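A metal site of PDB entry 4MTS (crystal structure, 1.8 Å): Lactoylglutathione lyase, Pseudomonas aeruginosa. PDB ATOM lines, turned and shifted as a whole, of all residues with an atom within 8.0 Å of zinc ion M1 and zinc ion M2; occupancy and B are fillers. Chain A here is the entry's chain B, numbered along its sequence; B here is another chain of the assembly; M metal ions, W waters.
N of Ala 76 lies within hydrogen-bond range of O of His 5 of chain B. OE1 of Glu 56 of chain B sits close to NE2 of His 5 of chain B. The backbone NH (N) of Glu 122 is in hydrogen-bond range of the backbone carbonyl oxygen (O) of Leu 75 (2.8 Å). N of Glu 56 of chain B lies within hydrogen-bond range of O of Ser 6 of chain B (2.8 Å). The backbone NH (N) of Ile 77 sits at hydrogen-bond distance from the backbone carbonyl oxygen (O) of Glu 122 (2.8 Å). N of Met 7 of chain B lies within hydrogen-bond range of O of His 74 (2.8 Å).
Zinc ion M2 is bound by the side-chain carboxylate of Glu 122 (2.1 Å), a ring nitrogen (NE2) of His 105 (2.2 Å), water W2 (2.3 Å) and water W1 (2.3 Å). Zinc ion M2 has four donor atoms within binding distance.
Zinc ion M1 is bound by water W2 (1.9 Å), OE1 of Glu 122 (1.9 Å), NE2 of His 5 of chain B (2.0 Å) and NE2 of His 74 (2.1 Å).
OE1 of Glu 56 of chain B touches zinc ion M1, 3.0 Å away. The nearest printed residue that does not touch zinc ion M1 is Ala 76 (4.05 Å).
Within 4 Å of zinc ion M2: His 105 and Glu 122. The nearest printed residue that does not touch zinc ion M2 is Gln 104 (4.1 Å).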
ATOM      1  N   GLY A  73      -3.755  -0.162  25.555  1.00  0.00           N
ATOM      2  CA  GLY A  73      -4.028  -1.479  26.135  1.00  0.00           C
ATOM      3  C   GLY A  73      -3.564  -1.624  27.562  1.00  0.00           C
ATOM      4  O   GLY A  73      -4.353  -1.452  28.492  1.00  0.00           O
ATOM      5  N   HIS A  74      -2.258  -1.921  27.730  1.00  0.00           N
ATOM      6  CA  HIS A  74      -1.667  -2.151  29.058  1.00  0.00           C
ATOM      7  C   HIS A  74      -0.158  -2.170  28.943  1.00  0.00           C
ATOM      8  O   HIS A  74       0.396  -2.079  27.845  1.00  0.00           O
ATOM      9  CB  HIS A  74      -2.149  -3.521  29.608  1.00  0.00           C
ATOM     10  CG  HIS A  74      -1.863  -4.689  28.705  1.00  0.00           C
ATOM     11  ND1 HIS A  74      -2.863  -5.239  27.895  1.00  0.00           N
ATOM     12  CD2 HIS A  74      -0.712  -5.386  28.509  1.00  0.00           C
ATOM     13  CE1 HIS A  74      -2.289  -6.241  27.246  1.00  0.00           C
ATOM     14  NE2 HIS A  74      -0.993  -6.344  27.537  1.00  0.00           N
ATOM     15  N   LEU A  75       0.501  -2.187  30.116  1.00  0.00           N
ATOM     16  CA  LEU A  75       1.930  -2.401  30.226  1.00  0.00           C
ATOM     17  C   LEU A  75       2.052  -3.769  30.880  1.00  0.00           C
ATOM     18  O   LEU A  75       1.381  -4.035  31.882  1.00  0.00           O
ATOM     19  CB  LEU A  75       2.548  -1.370  31.180  1.00  0.00           C
ATOM     20  CG  LEU A  75       4.082  -1.511  31.313  1.00  0.00           C
ATOM     21  CD1 LEU A  75       4.778  -1.070  30.006  1.00  0.00           C
ATOM     22  CD2 LEU A  75       4.538  -0.677  32.490  1.00  0.00           C
ATOM     23  N   ALA A  76       2.871  -4.642  30.334  1.00  0.00           N
ATOM     24  CA  ALA A  76       3.104  -5.976  30.912  1.00  0.00           C
ATOM     25  C   ALA A  76       4.434  -6.010  31.604  1.00  0.00           C
ATOM     26  O   ALA A  76       5.434  -5.507  31.082  1.00  0.00           O
ATOM     27  CB  ALA A  76       3.056  -7.046  29.825  1.00  0.00           C
ATOM     28  N   ILE A  77       4.438  -6.623  32.799  1.00  0.00           N
ATOM     29  CA  ILE A  77       5.647  -6.798  33.616  1.00  0.00           C
ATOM     30  C   ILE A  77       5.845  -8.294  33.958  1.00  0.00           C
ATOM     31  O   ILE A  77       4.889  -9.006  34.250  1.00  0.00           O
ATOM     32  CB  ILE A  77       5.528  -5.902  34.879  1.00  0.00           C
ATOM     33  CG1 ILE A  77       5.793  -4.435  34.438  1.00  0.00           C
ATOM     34  CG2 ILE A  77       6.525  -6.285  35.994  1.00  0.00           C
ATOM     35  CD1 ILE A  77       5.281  -3.452  35.426  1.00  0.00           C
ATOM     36  N   LEU A 102      -7.639 -16.740  28.090  1.00  0.00           N
ATOM     37  CA  LEU A 102      -7.031 -15.866  27.079  1.00  0.00           C
ATOM     38  C   LEU A 102      -6.183 -16.762  26.218  1.00  0.00           C
ATOM     39  O   LEU A 102      -5.233 -17.383  26.684  1.00  0.00           O
ATOM     40  CB  LEU A 102      -6.184 -14.711  27.691  1.00  0.00           C
ATOM     41  CG  LEU A 102      -6.938 -13.671  28.537  1.00  0.00           C
ATOM     42  CD1 LEU A 102      -5.944 -12.662  29.180  1.00  0.00           C
ATOM     43  CD2 LEU A 102      -8.033 -12.948  27.733  1.00  0.00           C
ATOM     44  N   GLN A 104      -3.985 -16.399  23.978  1.00  0.00           N
ATOM     45  CA  GLN A 104      -2.553 -16.156  23.817  1.00  0.00           C
ATOM     46  C   GLN A 104      -1.728 -16.527  25.064  1.00  0.00           C
ATOM     47  O   GLN A 104      -0.499 -16.344  25.062  1.00  0.00           O
ATOM     48  CB  GLN A 104      -2.330 -14.687  23.475  1.00  0.00           C
ATOM     49  CG  GLN A 104      -2.724 -13.706  24.593  1.00  0.00           C
ATOM     50  CD  GLN A 104      -4.139 -13.203  24.499  1.00  0.00           C
ATOM     51  OE1 GLN A 104      -5.117 -13.964  24.409  1.00  0.00           O
ATOM     52  NE2 GLN A 104      -4.283 -11.890  24.525  1.00  0.00           N
ATOM     53  N   HIS A 105      -2.414 -16.959  26.140  1.00  0.00           N
ATOM     54  CA  HIS A 105      -1.762 -17.277  27.394  1.00  0.00           C
ATOM     55  C   HIS A 105      -1.905 -18.755  27.815  1.00  0.00           C
ATOM     56  O   HIS A 105      -1.622 -19.106  28.973  1.00  0.00           O
ATOM     57  CB  HIS A 105      -2.231 -16.297  28.479  1.00  0.00           C
ATOM     58  CG  HIS A 105      -1.766 -14.897  28.244  1.00  0.00           C
ATOM     59  ND1 HIS A 105      -0.450 -14.530  28.454  1.00  0.00           N
ATOM     60  CD2 HIS A 105      -2.471 -13.794  27.883  1.00  0.00           C
ATOM     61  CE1 HIS A 105      -0.385 -13.236  28.168  1.00  0.00           C
ATOM     62  NE2 HIS A 105      -1.589 -12.754  27.831  1.00  0.00           N
ATOM     63  N   ILE A 110      -4.430 -14.942  33.826  1.00  0.00           N
ATOM     64  CA  ILE A 110      -3.608 -13.708  33.864  1.00  0.00           C
ATOM     65  C   ILE A 110      -4.205 -12.652  34.764  1.00  0.00           C
ATOM     66  O   ILE A 110      -5.381 -12.312  34.635  1.00  0.00           O
ATOM     67  CB  ILE A 110      -3.297 -13.177  32.431  1.00  0.00           C
ATOM     68  CG1 ILE A 110      -2.633 -14.246  31.540  1.00  0.00           C
ATOM     69  CG2 ILE A 110      -2.464 -11.865  32.454  1.00  0.00           C
ATOM     70  CD1 ILE A 110      -1.103 -14.666  31.911  1.00  0.00           C
ATOM     71  N   ALA A 111      -3.397 -12.140  35.699  1.00  0.00           N
ATOM     72  CA  ALA A 111      -3.779 -11.044  36.601  1.00  0.00           C
ATOM     73  C   ALA A 111      -3.409  -9.682  36.003  1.00  0.00           C
ATOM     74  O   ALA A 111      -2.350  -9.548  35.356  1.00  0.00           O
ATOM     75  CB  ALA A 111      -3.055 -11.194  37.929  1.00  0.00           C
ATOM     76  N   PHE A 112      -4.272  -8.683  36.220  1.00  0.00           N
ATOM     77  CA  PHE A 112      -4.060  -7.291  35.841  1.00  0.00           C
ATOM     78  C   PHE A 112      -4.241  -6.444  37.069  1.00  0.00           C
ATOM     79  O   PHE A 112      -5.188  -6.651  37.837  1.00  0.00           O
ATOM     80  CB  PHE A 112      -5.014  -6.802  34.752  1.00  0.00           C
ATOM     81  CG  PHE A 112      -4.894  -7.591  33.470  1.00  0.00           C
ATOM     82  CD1 PHE A 112      -5.489  -8.845  33.344  1.00  0.00           C
ATOM     83  CD2 PHE A 112      -4.169  -7.086  32.389  1.00  0.00           C
ATOM     84  CE1 PHE A 112      -5.326  -9.609  32.178  1.00  0.00           C
ATOM     85  CE2 PHE A 112      -4.085  -7.816  31.180  1.00  0.00           C
ATOM     86  CZ  PHE A 112      -4.638  -9.085  31.099  1.00  0.00           C
ATOM     87  N   VAL A 121      -1.974  -2.983  34.386  1.00  0.00           N
ATOM     88  CA  VAL A 121      -0.649  -3.584  34.380  1.00  0.00           C
ATOM     89  C   VAL A 121      -0.836  -5.101  34.344  1.00  0.00           C
ATOM     90  O   VAL A 121      -1.370  -5.688  35.283  1.00  0.00           O
ATOM     91  CB  VAL A 121       0.245  -3.130  35.582  1.00  0.00           C
ATOM     92  CG1 VAL A 121       1.596  -3.827  35.537  1.00  0.00           C
ATOM     93  CG2 VAL A 121       0.426  -1.604  35.573  1.00  0.00           C
ATOM     94  N   GLU A 122      -0.412  -5.722  33.274  1.00  0.00           N
ATOM     95  CA  GLU A 122      -0.485  -7.182  33.104  1.00  0.00           C
ATOM     96  C   GLU A 122       0.696  -7.855  33.781  1.00  0.00           C
ATOM     97  O   GLU A 122       1.871  -7.515  33.537  1.00  0.00           O
ATOM     98  CB  GLU A 122      -0.467  -7.477  31.601  1.00  0.00           C
ATOM     99  CG  GLU A 122      -0.521  -8.942  31.222  1.00  0.00           C
ATOM    100  CD  GLU A 122      -0.668  -9.170  29.731  1.00  0.00           C
ATOM    101  OE1 GLU A 122       0.226  -8.752  28.955  1.00  0.00           O
ATOM    102  OE2 GLU A 122      -1.742  -9.637  29.319  1.00  0.00           O
ATOM    103  N   LEU A 123       0.405  -8.856  34.588  1.00  0.00           N
ATOM    104  CA  LEU A 123       1.441  -9.618  35.282  1.00  0.00           C
ATOM    105  C   LEU A 123       1.705 -10.914  34.555  1.00  0.00           C
ATOM    106  O   LEU A 123       0.761 -11.676  34.324  1.00  0.00           O
ATOM    107  CB  LEU A 123       1.051  -9.882  36.744  1.00  0.00           C
ATOM    108  CG  LEU A 123       0.615  -8.657  37.566  1.00  0.00           C
ATOM    109  CD1 LEU A 123       0.286  -9.090  39.026  1.00  0.00           C
ATOM    110  CD2 LEU A 123       1.735  -7.587  37.625  1.00  0.00           C
ATOM    111  N   ILE A 124       2.954 -11.132  34.143  1.00  0.00           N
ATOM    112  CA  ILE A 124       3.336 -12.377  33.438  1.00  0.00           C
ATOM    113  C   ILE A 124       4.348 -13.098  34.331  1.00  0.00           C
ATOM    114  O   ILE A 124       5.405 -12.549  34.642  1.00  0.00           O
ATOM    115  CB  ILE A 124       3.861 -12.118  31.989  1.00  0.00           C
ATOM    116  CG1 ILE A 124       2.869 -11.347  31.085  1.00  0.00           C
ATOM    117  CG2 ILE A 124       4.416 -13.415  31.277  1.00  0.00           C
ATOM    118  CD1 ILE A 124       1.549 -11.940  30.843  1.00  0.00           C
ATOM    119  N   LEU B   4       7.932  -6.068  30.007  1.00  0.00           N
ATOM    120  CA  LEU B   4       7.863  -6.994  28.863  1.00  0.00           C
ATOM    121  C   LEU B   4       7.345  -6.312  27.591  1.00  0.00           C
ATOM    122  O   LEU B   4       7.912  -6.541  26.527  1.00  0.00           O
ATOM    123  CB  LEU B   4       6.967  -8.188  29.187  1.00  0.00           C
ATOM    124  CG  LEU B   4       7.470  -9.133  30.281  1.00  0.00           C
ATOM    125  CD1 LEU B   4       6.415 -10.118  30.629  1.00  0.00           C
ATOM    126  CD2 LEU B   4       8.694  -9.881  29.833  1.00  0.00           C
ATOM    127  N   HIS B   5       6.247  -5.526  27.691  1.00  0.00           N
ATOM    128  CA  HIS B   5       5.696  -4.883  26.505  1.00  0.00           C
ATOM    129  C   HIS B   5       4.647  -3.851  26.855  1.00  0.00           C
ATOM    130  O   HIS B   5       4.184  -3.792  27.980  1.00  0.00           O
ATOM    131  CB  HIS B   5       5.060  -5.911  25.487  1.00  0.00           C
ATOM    132  CG  HIS B   5       3.972  -6.786  26.066  1.00  0.00           C
ATOM    133  ND1 HIS B   5       4.249  -8.085  26.488  1.00  0.00           N
ATOM    134  CD2 HIS B   5       2.647  -6.552  26.214  1.00  0.00           C
ATOM    135  CE1 HIS B   5       3.095  -8.579  26.898  1.00  0.00           C
ATOM    136  NE2 HIS B   5       2.103  -7.725  26.749  1.00  0.00           N
ATOM    137  N   SER B   6       4.370  -2.976  25.891  1.00  0.00           N
ATOM    138  CA  SER B   6       3.287  -1.998  25.969  1.00  0.00           C
ATOM    139  C   SER B   6       2.355  -2.457  24.860  1.00  0.00           C
ATOM    140  O   SER B   6       2.823  -2.756  23.744  1.00  0.00           O
ATOM    141  CB  SER B   6       3.810  -0.614  25.610  1.00  0.00           C
ATOM    142  OG  SER B   6       2.748   0.317  25.639  1.00  0.00           O
ATOM    143  N   MET B   7       1.055  -2.496  25.130  1.00  0.00           N
ATOM    144  CA  MET B   7       0.068  -2.946  24.139  1.00  0.00           C
ATOM    145  C   MET B   7      -0.820  -1.814  23.657  1.00  0.00           C
ATOM    146  O   MET B   7      -1.327  -1.071  24.473  1.00  0.00           O
ATOM    147  CB  MET B   7      -0.786  -4.111  24.688  1.00  0.00           C
ATOM    148  CG  MET B   7      -1.710  -4.733  23.602  1.00  0.00           C
ATOM    149  SD  MET B   7      -3.269  -3.871  23.312  1.00  0.00           S
ATOM    150  CE  MET B   7      -4.286  -4.697  24.486  1.00  0.00           C
ATOM    151  N   ARG B  30       6.850 -11.863  16.748  1.00  0.00           N
ATOM    152  CA  ARG B  30       5.869 -12.918  16.912  1.00  0.00           C
ATOM    153  C   ARG B  30       4.505 -12.377  16.437  1.00  0.00           C
ATOM    154  O   ARG B  30       4.135 -11.236  16.728  1.00  0.00           O
ATOM    155  CB  ARG B  30       5.839 -13.255  18.449  1.00  0.00           C
ATOM    156  CG  ARG B  30       4.783 -14.252  18.924  1.00  0.00           C
ATOM    157  CD  ARG B  30       5.109 -14.837  20.285  1.00  0.00           C
ATOM    158  NE  ARG B  30       5.239 -13.806  21.339  1.00  0.00           N
ATOM    159  CZ  ARG B  30       4.391 -13.674  22.355  1.00  0.00           C
ATOM    160  NH1 ARG B  30       3.338 -14.473  22.467  1.00  0.00           N
ATOM    161  NH2 ARG B  30       4.593 -12.721  23.265  1.00  0.00           N
ATOM    162  N   PHE B  39      -9.231 -12.266  16.901  1.00  0.00           N
ATOM    163  CA  PHE B  39      -8.266 -11.184  17.120  1.00  0.00           C
ATOM    164  C   PHE B  39      -6.909 -11.662  16.725  1.00  0.00           C
ATOM    165  O   PHE B  39      -6.696 -12.872  16.632  1.00  0.00           O
ATOM    166  CB  PHE B  39      -8.295 -10.654  18.569  1.00  0.00           C
ATOM    167  CG  PHE B  39      -7.724 -11.588  19.599  1.00  0.00           C
ATOM    168  CD1 PHE B  39      -8.504 -12.604  20.146  1.00  0.00           C
ATOM    169  CD2 PHE B  39      -6.421 -11.443  20.044  1.00  0.00           C
ATOM    170  CE1 PHE B  39      -7.970 -13.492  21.069  1.00  0.00           C
ATOM    171  CE2 PHE B  39      -5.907 -12.311  20.997  1.00  0.00           C
ATOM    172  CZ  PHE B  39      -6.676 -13.318  21.510  1.00  0.00           C
ATOM    173  N   LEU B  41      -2.606 -10.720  17.492  1.00  0.00           N
ATOM    174  CA  LEU B  41      -1.594  -9.999  18.268  1.00  0.00           C
ATOM    175  C   LEU B  41      -0.337  -9.974  17.432  1.00  0.00           C
ATOM    176  O   LEU B  41      -0.018 -10.952  16.733  1.00  0.00           O
ATOM    177  CB  LEU B  41      -1.217 -10.764  19.552  1.00  0.00           C
ATOM    178  CG  LEU B  41      -2.248 -11.296  20.443  1.00  0.00           C
ATOM    179  CD1 LEU B  41      -1.581 -12.047  21.564  1.00  0.00           C
ATOM    180  CD2 LEU B  41      -3.139 -10.154  20.973  1.00  0.00           C
ATOM    181  N   PHE B  43       3.863  -8.713  17.943  1.00  0.00           N
ATOM    182  CA  PHE B  43       4.900  -8.115  18.788  1.00  0.00           C
ATOM    183  C   PHE B  43       5.997  -7.664  17.835  1.00  0.00           C
ATOM    184  O   PHE B  43       6.500  -8.441  17.005  1.00  0.00           O
ATOM    185  CB  PHE B  43       5.403  -9.129  19.846  1.00  0.00           C
ATOM    186  CG  PHE B  43       4.364  -9.497  20.893  1.00  0.00           C
ATOM    187  CD1 PHE B  43       3.408 -10.471  20.644  1.00  0.00           C
ATOM    188  CD2 PHE B  43       4.395  -8.903  22.164  1.00  0.00           C
ATOM    189  CE1 PHE B  43       2.465 -10.821  21.638  1.00  0.00           C
ATOM    190  CE2 PHE B  43       3.435  -9.224  23.130  1.00  0.00           C
ATOM    191  CZ  PHE B  43       2.473 -10.175  22.853  1.00  0.00           C
ATOM    192  N   GLU B  56       3.395  -4.400  21.584  1.00  0.00           N
ATOM    193  CA  GLU B  56       2.377  -5.369  21.175  1.00  0.00           C
ATOM    194  C   GLU B  56       1.263  -4.602  20.488  1.00  0.00           C
ATOM    195  O   GLU B  56       0.698  -3.682  21.071  1.00  0.00           O
ATOM    196  CB  GLU B  56       1.804  -6.081  22.405  1.00  0.00           C
ATOM    197  CG  GLU B  56       0.783  -7.127  21.964  1.00  0.00           C
ATOM    198  CD  GLU B  56       0.064  -7.817  23.089  1.00  0.00           C
ATOM    199  OE1 GLU B  56       0.231  -7.392  24.263  1.00  0.00           O
ATOM    200  OE2 GLU B  56      -0.619  -8.833  22.807  1.00  0.00           O
ATOM    201  N   THR B  58      -2.591  -5.076  18.855  1.00  0.00           N
ATOM    202  CA  THR B  58      -3.774  -5.960  18.892  1.00  0.00           C
ATOM    203  C   THR B  58      -4.804  -5.468  17.881  1.00  0.00           C
ATOM    204  O   THR B  58      -5.055  -4.266  17.778  1.00  0.00           O
ATOM    205  CB  THR B  58      -4.395  -6.008  20.305  1.00  0.00           C
ATOM    206  OG1 THR B  58      -3.406  -6.378  21.271  1.00  0.00           O
ATOM    207  CG2 THR B  58      -5.559  -6.978  20.402  1.00  0.00           C
HETATM  208 ZN    ZN M   1       0.152  -8.025  27.182  1.00  0.00          ZN
HETATM  209 ZN    ZN M   2      -1.758 -10.598  27.468  1.00  0.00          ZN
HETATM  210  O   HOH W   1      -3.940 -10.033  27.171  1.00  0.00           O
HETATM  211  O   HOH W   2      -0.816  -9.161  25.996  1.00  0.00           O
